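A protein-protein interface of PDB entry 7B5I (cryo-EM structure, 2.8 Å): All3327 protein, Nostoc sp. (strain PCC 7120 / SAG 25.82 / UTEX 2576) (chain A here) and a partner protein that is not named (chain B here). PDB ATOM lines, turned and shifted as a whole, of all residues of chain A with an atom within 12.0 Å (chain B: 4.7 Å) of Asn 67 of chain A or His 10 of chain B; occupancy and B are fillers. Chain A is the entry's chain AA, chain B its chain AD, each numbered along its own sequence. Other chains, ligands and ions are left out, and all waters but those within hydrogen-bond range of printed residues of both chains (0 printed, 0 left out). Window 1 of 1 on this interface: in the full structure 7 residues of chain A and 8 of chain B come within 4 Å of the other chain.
A ring nitrogen (NE2) of His 98 of chain B lies within hydrogen-bond range of the side-chain amide oxygen (OD1) of Asn 82 of chain A, at 3.2 Å.
The side-chain amide oxygen of Asn 67 of chain A lies within hydrogen-bond range of a ring nitrogen (ND1) of His 10 of chain B.
The backbone carbonyl oxygen (O) of His 10 of chain B lies within hydrogen-bond range of the backbone NH (N) of Leu 94 of chain B, 2.9 Å away.
A ring nitrogen (ND1) of His 98 of chain B sits at hydrogen-bond distance from a ring nitrogen (NE2) of His 10 of chain B (3.0 Å).
N of His 98 of chain B is in hydrogen-bond range of OD1 of Asn 95 of chain B (3.4 Å).
The side-chain amide nitrogen of Asn 82 of chain A sits at hydrogen-bond distance from the side-chain amide oxygen of Gln 179 of chain A, 3.1 Å away.
Among the printed residues, pairs that only touch across the chains: Asn 67 of chain A with Phe 11 of chain B, Asn 67 of chain A with Phe 9 of chain B, Asn 67 of chain A with Phe 22 of chain B and Asn 67 of chain A with Gly 21 of chain B.
Asn 67 of chain A touches five residues of chain B.
His 10 of chain B touches just one residue of chain A: Asn 67.
Phe 9 of chain B touches just one residue of chain A: Asn 67.
No residue of chain A comes within 4 Å of Leu 93 of chain B.
Leu 94 of chain B touches none of the printed residues of chain A.
Of the printed residues of chain B, Asn 82 of chain A touches His 98 (3.2 Å).
Printed residues of chain A within 4 Å of Phe 22 of chain B: Asn 67.
The nearest printed residue of chain B that does not touch Asn 67 of chain A is Leu 94 of chain B (6.2 Å).
The nearest printed residue of chain A that does not touch Phe 22 of chain B is Lys 66 of chain A (5.4 Å).
Of the 10 printed residues of chain B, 6 touch a printed residue of chain A.
Hydrophobic or aromatic side chains of chain B that line the printed part of chain A: His 10, Phe 11 and His 98.
Along chain B the printed residues that touch a printed residue of chain A span positions 9 to 98.
Of the 19 printed residues of chain A, 2 touch a printed residue of chain B.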
ATOM      1  N   GLU A  61      37.853  29.263  35.211  1.00  0.00           N
ATOM      2  CA  GLU A  61      36.700  28.387  35.092  1.00  0.00           C
ATOM      3  C   GLU A  61      37.103  26.936  35.317  1.00  0.00           C
ATOM      4  O   GLU A  61      38.214  26.523  34.983  1.00  0.00           O
ATOM      5  CB  GLU A  61      36.055  28.535  33.716  1.00  0.00           C
ATOM      6  CG  GLU A  61      34.715  27.850  33.594  1.00  0.00           C
ATOM      7  CD  GLU A  61      34.077  28.052  32.242  1.00  0.00           C
ATOM      8  OE1 GLU A  61      34.778  28.508  31.318  1.00  0.00           O
ATOM      9  OE2 GLU A  61      32.874  27.751  32.101  1.00  0.00           O
ATOM     10  N   GLU A  62      36.186  26.161  35.884  1.00  0.00           N
ATOM     11  CA  GLU A  62      36.416  24.742  36.130  1.00  0.00           C
ATOM     12  C   GLU A  62      36.041  23.957  34.878  1.00  0.00           C
ATOM     13  O   GLU A  62      34.875  23.938  34.474  1.00  0.00           O
ATOM     14  CB  GLU A  62      35.620  24.267  37.340  1.00  0.00           C
ATOM     15  CG  GLU A  62      35.762  22.781  37.613  1.00  0.00           C
ATOM     16  CD  GLU A  62      37.210  22.326  37.631  1.00  0.00           C
ATOM     17  OE1 GLU A  62      38.025  22.940  38.351  1.00  0.00           O
ATOM     18  OE2 GLU A  62      37.537  21.352  36.924  1.00  0.00           O
ATOM     19  N   THR A  63      37.026  23.294  34.278  1.00  0.00           N
ATOM     20  CA  THR A  63      36.833  22.590  33.017  1.00  0.00           C
ATOM     21  C   THR A  63      36.032  21.303  33.168  1.00  0.00           C
ATOM     22  O   THR A  63      35.422  20.851  32.195  1.00  0.00           O
ATOM     23  CB  THR A  63      38.197  22.282  32.392  1.00  0.00           C
ATOM     24  OG1 THR A  63      38.960  23.490  32.302  1.00  0.00           O
ATOM     25  CG2 THR A  63      38.050  21.698  30.998  1.00  0.00           C
ATOM     26  N   THR A  64      35.985  20.723  34.361  1.00  0.00           N
ATOM     27  CA  THR A  64      35.329  19.437  34.535  1.00  0.00           C
ATOM     28  C   THR A  64      33.810  19.553  34.553  1.00  0.00           C
ATOM     29  O   THR A  64      33.123  18.590  34.197  1.00  0.00           O
ATOM     30  CB  THR A  64      35.840  18.779  35.819  1.00  0.00           C
ATOM     31  OG1 THR A  64      37.248  18.549  35.696  1.00  0.00           O
ATOM     32  CG2 THR A  64      35.163  17.452  36.066  1.00  0.00           C
ATOM     33  N   LEU A  65      33.272  20.715  34.905  1.00  0.00           N
ATOM     34  CA  LEU A  65      31.832  20.898  35.018  1.00  0.00           C
ATOM     35  C   LEU A  65      31.213  21.520  33.774  1.00  0.00           C
ATOM     36  O   LEU A  65      30.018  21.827  33.778  1.00  0.00           O
ATOM     37  CB  LEU A  65      31.506  21.741  36.248  1.00  0.00           C
ATOM     38  CG  LEU A  65      31.916  21.103  37.570  1.00  0.00           C
ATOM     39  CD1 LEU A  65      31.565  22.009  38.727  1.00  0.00           C
ATOM     40  CD2 LEU A  65      31.256  19.753  37.727  1.00  0.00           C
ATOM     41  N   LYS A  66      31.989  21.722  32.717  1.00  0.00           N
ATOM     42  CA  LYS A  66      31.407  22.102  31.444  1.00  0.00           C
ATOM     43  C   LYS A  66      30.624  20.935  30.854  1.00  0.00           C
ATOM     44  O   LYS A  66      30.791  19.778  31.250  1.00  0.00           O
ATOM     45  CB  LYS A  66      32.490  22.541  30.466  1.00  0.00           C
ATOM     46  CG  LYS A  66      33.015  23.934  30.688  1.00  0.00           C
ATOM     47  CD  LYS A  66      34.115  24.232  29.692  1.00  0.00           C
ATOM     48  CE  LYS A  66      34.437  25.706  29.645  1.00  0.00           C
ATOM     49  NZ  LYS A  66      33.351  26.471  28.982  1.00  0.00           N
ATOM     50  N   ASN A  67      29.757  21.254  29.896  1.00  0.00           N
ATOM     51  CA  ASN A  67      28.948  20.253  29.201  1.00  0.00           C
ATOM     52  C   ASN A  67      27.995  19.538  30.155  1.00  0.00           C
ATOM     53  O   ASN A  67      27.818  18.324  30.078  1.00  0.00           O
ATOM     54  CB  ASN A  67      29.816  19.237  28.456  1.00  0.00           C
ATOM     55  CG  ASN A  67      30.657  19.862  27.367  1.00  0.00           C
ATOM     56  OD1 ASN A  67      30.239  20.806  26.702  1.00  0.00           O
ATOM     57  ND2 ASN A  67      31.853  19.330  27.176  1.00  0.00           N
ATOM     58  N   SER A  68      27.391  20.282  31.055  1.00  0.00           N
ATOM     59  CA  SER A  68      26.324  19.765  31.894  1.00  0.00           C
ATOM     60  C   SER A  68      24.983  19.952  31.195  1.00  0.00           C
ATOM     61  O   SER A  68      24.856  20.790  30.301  1.00  0.00           O
ATOM     62  CB  SER A  68      26.340  20.473  33.245  1.00  0.00           C
ATOM     63  OG  SER A  68      26.065  21.851  33.096  1.00  0.00           O
ATOM     64  N   PRO A  69      23.964  19.173  31.566  1.00  0.00           N
ATOM     65  CA  PRO A  69      22.705  19.191  30.808  1.00  0.00           C
ATOM     66  C   PRO A  69      22.045  20.562  30.790  1.00  0.00           C
ATOM     67  O   PRO A  69      22.203  21.366  31.708  1.00  0.00           O
ATOM     68  CB  PRO A  69      21.836  18.170  31.548  1.00  0.00           C
ATOM     69  CG  PRO A  69      22.809  17.261  32.193  1.00  0.00           C
ATOM     70  CD  PRO A  69      23.956  18.124  32.599  1.00  0.00           C
ATOM     71  N   HIS A  70      21.288  20.818  29.721  1.00  0.00           N
ATOM     72  CA  HIS A  70      20.622  22.099  29.525  1.00  0.00           C
ATOM     73  C   HIS A  70      19.104  22.003  29.660  1.00  0.00           C
ATOM     74  O   HIS A  70      18.391  22.906  29.220  1.00  0.00           O
ATOM     75  CB  HIS A  70      20.995  22.692  28.165  1.00  0.00           C
ATOM     76  CG  HIS A  70      20.374  21.991  26.995  1.00  0.00           C
ATOM     77  ND1 HIS A  70      20.759  20.733  26.587  1.00  0.00           N
ATOM     78  CD2 HIS A  70      19.392  22.376  26.146  1.00  0.00           C
ATOM     79  CE1 HIS A  70      20.042  20.373  25.537  1.00  0.00           C
ATOM     80  NE2 HIS A  70      19.204  21.352  25.251  1.00  0.00           N
ATOM     81  N   TYR A  71      18.593  20.938  30.273  1.00  0.00           N
ATOM     82  CA  TYR A  71      17.161  20.809  30.486  1.00  0.00           C
ATOM     83  C   TYR A  71      16.909  20.071  31.794  1.00  0.00           C
ATOM     84  O   TYR A  71      17.807  19.444  32.359  1.00  0.00           O
ATOM     85  CB  TYR A  71      16.484  20.080  29.321  1.00  0.00           C
ATOM     86  CG  TYR A  71      16.707  18.592  29.331  1.00  0.00           C
ATOM     87  CD1 TYR A  71      17.821  18.038  28.726  1.00  0.00           C
ATOM     88  CD2 TYR A  71      15.808  17.739  29.951  1.00  0.00           C
ATOM     89  CE1 TYR A  71      18.033  16.680  28.738  1.00  0.00           C
ATOM     90  CE2 TYR A  71      16.014  16.382  29.970  1.00  0.00           C
ATOM     91  CZ  TYR A  71      17.126  15.858  29.362  1.00  0.00           C
ATOM     92  OH  TYR A  71      17.330  14.502  29.375  1.00  0.00           O
ATOM     93  N   TYR A  80      13.738  24.227  29.798  1.00  0.00           N
ATOM     94  CA  TYR A  80      15.016  24.512  29.162  1.00  0.00           C
ATOM     95  C   TYR A  80      15.624  25.761  29.779  1.00  0.00           C
ATOM     96  O   TYR A  80      14.969  26.809  29.832  1.00  0.00           O
ATOM     97  CB  TYR A  80      14.853  24.724  27.657  1.00  0.00           C
ATOM     98  CG  TYR A  80      14.373  23.519  26.895  1.00  0.00           C
ATOM     99  CD1 TYR A  80      15.258  22.541  26.481  1.00  0.00           C
ATOM    100  CD2 TYR A  80      13.037  23.373  26.568  1.00  0.00           C
ATOM    101  CE1 TYR A  80      14.822  21.443  25.779  1.00  0.00           C
ATOM    102  CE2 TYR A  80      12.593  22.282  25.867  1.00  0.00           C
ATOM    103  CZ  TYR A  80      13.486  21.320  25.476  1.00  0.00           C
ATOM    104  OH  TYR A  80      13.042  20.226  24.775  1.00  0.00           O
ATOM    105  N   GLN A  81      16.878  25.642  30.218  1.00  0.00           N
ATOM    106  CA  GLN A  81      17.646  26.721  30.821  1.00  0.00           C
ATOM    107  C   GLN A  81      19.130  26.442  30.606  1.00  0.00           C
ATOM    108  O   GLN A  81      19.553  25.286  30.560  1.00  0.00           O
ATOM    109  CB  GLN A  81      17.335  26.852  32.317  1.00  0.00           C
ATOM    110  CG  GLN A  81      18.066  27.981  33.009  1.00  0.00           C
ATOM    111  CD  GLN A  81      17.794  28.023  34.495  1.00  0.00           C
ATOM    112  OE1 GLN A  81      16.946  27.295  35.001  1.00  0.00           O
ATOM    113  NE2 GLN A  81      18.519  28.878  35.204  1.00  0.00           N
ATOM    114  N   ASN A  82      19.922  27.513  30.470  1.00  0.00           N
ATOM    115  CA  ASN A  82      21.355  27.351  30.240  1.00  0.00           C
ATOM    116  C   ASN A  82      22.070  26.991  31.541  1.00  0.00           C
ATOM    117  O   ASN A  82      21.688  27.469  32.611  1.00  0.00           O
ATOM    118  CB  ASN A  82      21.965  28.626  29.662  1.00  0.00           C
ATOM    119  CG  ASN A  82      21.521  28.898  28.238  1.00  0.00           C
ATOM    120  OD1 ASN A  82      21.386  27.983  27.432  1.00  0.00           O
ATOM    121  ND2 ASN A  82      21.307  30.168  27.920  1.00  0.00           N
ATOM    122  N   PRO A  83      23.110  26.163  31.475  1.00  0.00           N
ATOM    123  CA  PRO A  83      23.820  25.741  32.694  1.00  0.00           C
ATOM    124  C   PRO A  83      24.602  26.889  33.306  1.00  0.00           C
ATOM    125  O   PRO A  83      24.901  27.880  32.625  1.00  0.00           O
ATOM    126  CB  PRO A  83      24.760  24.637  32.185  1.00  0.00           C
ATOM    127  CG  PRO A  83      24.199  24.222  30.870  1.00  0.00           C
ATOM    128  CD  PRO A  83      23.595  25.450  30.285  1.00  0.00           C
ATOM    129  N   PRO A  84      24.955  26.796  34.584  1.00  0.00           N
ATOM    130  CA  PRO A  84      25.669  27.892  35.245  1.00  0.00           C
ATOM    131  C   PRO A  84      27.162  27.860  34.944  1.00  0.00           C
ATOM    132  O   PRO A  84      27.680  26.949  34.303  1.00  0.00           O
ATOM    133  CB  PRO A  84      25.400  27.630  36.726  1.00  0.00           C
ATOM    134  CG  PRO A  84      25.277  26.163  36.808  1.00  0.00           C
ATOM    135  CD  PRO A  84      24.626  25.714  35.527  1.00  0.00           C
ATOM    136  N   VAL A  85      27.853  28.887  35.433  1.00  0.00           N
ATOM    137  CA  VAL A  85      29.291  29.048  35.249  1.00  0.00           C
ATOM    138  C   VAL A  85      29.975  28.837  36.592  1.00  0.00           C
ATOM    139  O   VAL A  85      29.618  29.482  37.582  1.00  0.00           O
ATOM    140  CB  VAL A  85      29.630  30.431  34.667  1.00  0.00           C
ATOM    141  CG1 VAL A  85      31.111  30.538  34.371  1.00  0.00           C
ATOM    142  CG2 VAL A  85      28.821  30.687  33.412  1.00  0.00           C
ATOM    143  N   ASN A  86      30.961  27.945  36.624  1.00  0.00           N
ATOM    144  CA  ASN A  86      31.652  27.558  37.849  1.00  0.00           C
ATOM    145  C   ASN A  86      33.073  28.102  37.834  1.00  0.00           C
ATOM    146  O   ASN A  86      33.811  27.887  36.869  1.00  0.00           O
ATOM    147  CB  ASN A  86      31.668  26.038  37.995  1.00  0.00           C
ATOM    148  CG  ASN A  86      30.292  25.430  37.865  1.00  0.00           C
ATOM    149  OD1 ASN A  86      29.506  25.439  38.809  1.00  0.00           O
ATOM    150  ND2 ASN A  86      29.991  24.902  36.690  1.00  0.00           N
ATOM    151  N   GLN A 179      14.485  29.529  29.778  1.00  0.00           N
ATOM    152  CA  GLN A 179      14.677  29.614  28.340  1.00  0.00           C
ATOM    153  C   GLN A 179      13.484  29.107  27.547  1.00  0.00           C
ATOM    154  O   GLN A 179      13.009  29.814  26.657  1.00  0.00           O
ATOM    155  CB  GLN A 179      15.943  28.859  27.927  1.00  0.00           C
ATOM    156  CG  GLN A 179      16.325  29.054  26.486  1.00  0.00           C
ATOM    157  CD  GLN A 179      17.789  28.798  26.258  1.00  0.00           C
ATOM    158  OE1 GLN A 179      18.624  29.672  26.473  1.00  0.00           O
ATOM    159  NE2 GLN A 179      18.114  27.586  25.834  1.00  0.00           N
ATOM    160  N   LYS B   8      35.314  23.841  18.928  1.00  0.00           N
ATOM    161  CA  LYS B   8      35.402  22.449  19.343  1.00  0.00           C
ATOM    162  C   LYS B   8      35.366  22.247  20.842  1.00  0.00           C
ATOM    163  O   LYS B   8      36.153  21.470  21.383  1.00  0.00           O
ATOM    164  CB  LYS B   8      36.663  21.799  18.764  1.00  0.00           C
ATOM    165  CG  LYS B   8      37.962  22.372  19.305  1.00  0.00           C
ATOM    166  CD  LYS B   8      39.167  21.630  18.750  1.00  0.00           C
ATOM    167  CE  LYS B   8      40.462  22.150  19.354  1.00  0.00           C
ATOM    168  NZ  LYS B   8      41.649  21.409  18.844  1.00  0.00           N
ATOM    169  N   PHE B   9      34.460  22.936  21.524  1.00  0.00           N
ATOM    170  CA  PHE B   9      34.383  22.742  22.968  1.00  0.00           C
ATOM    171  C   PHE B   9      32.980  22.525  23.530  1.00  0.00           C
ATOM    172  O   PHE B   9      32.805  22.631  24.746  1.00  0.00           O
ATOM    173  CB  PHE B   9      35.034  23.921  23.700  1.00  0.00           C
ATOM    174  CG  PHE B   9      34.420  25.251  23.389  1.00  0.00           C
ATOM    175  CD1 PHE B   9      33.260  25.665  24.018  1.00  0.00           C
ATOM    176  CD2 PHE B   9      35.015  26.101  22.482  1.00  0.00           C
ATOM    177  CE1 PHE B   9      32.702  26.888  23.732  1.00  0.00           C
ATOM    178  CE2 PHE B   9      34.461  27.325  22.202  1.00  0.00           C
ATOM    179  CZ  PHE B   9      33.305  27.717  22.825  1.00  0.00           C
ATOM    180  N   HIS B  10      31.983  22.205  22.709  1.00  0.00           N
ATOM    181  CA  HIS B  10      30.611  22.019  23.187  1.00  0.00           C
ATOM    182  C   HIS B  10      30.039  20.770  22.520  1.00  0.00           C
ATOM    183  O   HIS B  10      29.617  20.822  21.363  1.00  0.00           O
ATOM    184  CB  HIS B  10      29.784  23.266  22.885  1.00  0.00           C
ATOM    185  CG  HIS B  10      28.483  23.340  23.615  1.00  0.00           C
ATOM    186  ND1 HIS B  10      28.278  22.718  24.827  1.00  0.00           N
ATOM    187  CD2 HIS B  10      27.331  23.986  23.331  1.00  0.00           C
ATOM    188  CE1 HIS B  10      27.055  22.968  25.247  1.00  0.00           C
ATOM    189  NE2 HIS B  10      26.456  23.738  24.355  1.00  0.00           N
ATOM    190  N   PHE B  11      30.021  19.655  23.249  1.00  0.00           N
ATOM    191  CA  PHE B  11      29.694  18.350  22.686  1.00  0.00           C
ATOM    192  C   PHE B  11      29.040  17.478  23.751  1.00  0.00           C
ATOM    193  O   PHE B  11      28.982  17.842  24.923  1.00  0.00           O
ATOM    194  CB  PHE B  11      30.950  17.674  22.124  1.00  0.00           C
ATOM    195  CG  PHE B  11      32.066  17.538  23.121  1.00  0.00           C
ATOM    196  CD1 PHE B  11      32.967  18.567  23.326  1.00  0.00           C
ATOM    197  CD2 PHE B  11      32.219  16.374  23.845  1.00  0.00           C
ATOM    198  CE1 PHE B  11      33.987  18.436  24.240  1.00  0.00           C
ATOM    199  CE2 PHE B  11      33.238  16.241  24.755  1.00  0.00           C
ATOM    200  CZ  PHE B  11      34.123  17.271  24.954  1.00  0.00           C
ATOM    201  N   GLY B  21      29.393  14.570  30.860  1.00  0.00           N
ATOM    202  CA  GLY B  21      30.387  15.596  31.116  1.00  0.00           C
ATOM    203  C   GLY B  21      31.806  15.097  30.929  1.00  0.00           C
ATOM    204  O   GLY B  21      32.565  14.980  31.891  1.00  0.00           O
ATOM    205  N   PHE B  22      32.165  14.803  29.684  1.00  0.00           N
ATOM    206  CA  PHE B  22      33.503  14.317  29.367  1.00  0.00           C
ATOM    207  C   PHE B  22      34.438  15.463  29.001  1.00  0.00           C
ATOM    208  O   PHE B  22      34.005  16.484  28.467  1.00  0.00           O
ATOM    209  CB  PHE B  22      33.448  13.301  28.223  1.00  0.00           C
ATOM    210  CG  PHE B  22      32.784  12.005  28.593  1.00  0.00           C
ATOM    211  CD1 PHE B  22      33.529  10.944  29.078  1.00  0.00           C
ATOM    212  CD2 PHE B  22      31.415  11.849  28.454  1.00  0.00           C
ATOM    213  CE1 PHE B  22      32.922   9.749  29.418  1.00  0.00           C
ATOM    214  CE2 PHE B  22      30.800  10.658  28.793  1.00  0.00           C
ATOM    215  CZ  PHE B  22      31.556   9.606  29.275  1.00  0.00           C
ATOM    216  N   LEU B  93      28.205  17.006  18.243  1.00  0.00           N
ATOM    217  CA  LEU B  93      28.767  18.337  18.437  1.00  0.00           C
ATOM    218  C   LEU B  93      27.627  19.347  18.443  1.00  0.00           C
ATOM    219  O   LEU B  93      26.931  19.509  17.437  1.00  0.00           O
ATOM    220  CB  LEU B  93      29.780  18.659  17.340  1.00  0.00           C
ATOM    221  CG  LEU B  93      30.442  20.032  17.352  1.00  0.00           C
ATOM    222  CD1 LEU B  93      31.431  20.119  18.481  1.00  0.00           C
ATOM    223  CD2 LEU B  93      31.143  20.286  16.044  1.00  0.00           C
ATOM    224  N   LEU B  94      27.546  20.190  19.446  1.00  0.00           N
ATOM    225  CA  LEU B  94      26.468  21.154  19.497  1.00  0.00           C
ATOM    226  C   LEU B  94      26.889  22.568  19.222  1.00  0.00           C
ATOM    227  O   LEU B  94      28.013  22.936  19.439  1.00  0.00           O
ATOM    228  CB  LEU B  94      25.825  21.126  20.866  1.00  0.00           C
ATOM    229  CG  LEU B  94      25.648  19.781  21.522  1.00  0.00           C
ATOM    230  CD1 LEU B  94      25.338  20.002  22.973  1.00  0.00           C
ATOM    231  CD2 LEU B  94      24.586  18.948  20.864  1.00  0.00           C
ATOM    232  N   ASN B  95      25.987  23.368  18.709  1.00  0.00           N
ATOM    233  CA  ASN B  95      26.299  24.760  18.497  1.00  0.00           C
ATOM    234  C   ASN B  95      25.677  25.632  19.582  1.00  0.00           C
ATOM    235  O   ASN B  95      25.011  25.124  20.455  1.00  0.00           O
ATOM    236  CB  ASN B  95      25.843  25.257  17.133  1.00  0.00           C
ATOM    237  CG  ASN B  95      24.366  25.371  17.012  1.00  0.00           C
ATOM    238  OD1 ASN B  95      23.663  25.290  17.977  1.00  0.00           O
ATOM    239  ND2 ASN B  95      23.907  25.635  15.824  1.00  0.00           N
ATOM    240  N   HIS B  98      22.475  24.763  21.131  1.00  0.00           N
ATOM    241  CA  HIS B  98      22.472  23.350  21.503  1.00  0.00           C
ATOM    242  C   HIS B  98      21.786  22.391  20.528  1.00  0.00           C
ATOM    243  O   HIS B  98      21.084  21.478  20.959  1.00  0.00           O
ATOM    244  CB  HIS B  98      21.897  23.168  22.913  1.00  0.00           C
ATOM    245  CG  HIS B  98      22.279  24.256  23.867  1.00  0.00           C
ATOM    246  ND1 HIS B  98      23.461  24.243  24.576  1.00  0.00           N
ATOM    247  CD2 HIS B  98      21.637  25.391  24.229  1.00  0.00           C
ATOM    248  CE1 HIS B  98      23.530  25.323  25.334  1.00  0.00           C
ATOM    249  NE2 HIS B  98      22.435  26.036  25.142  1.00  0.00           N
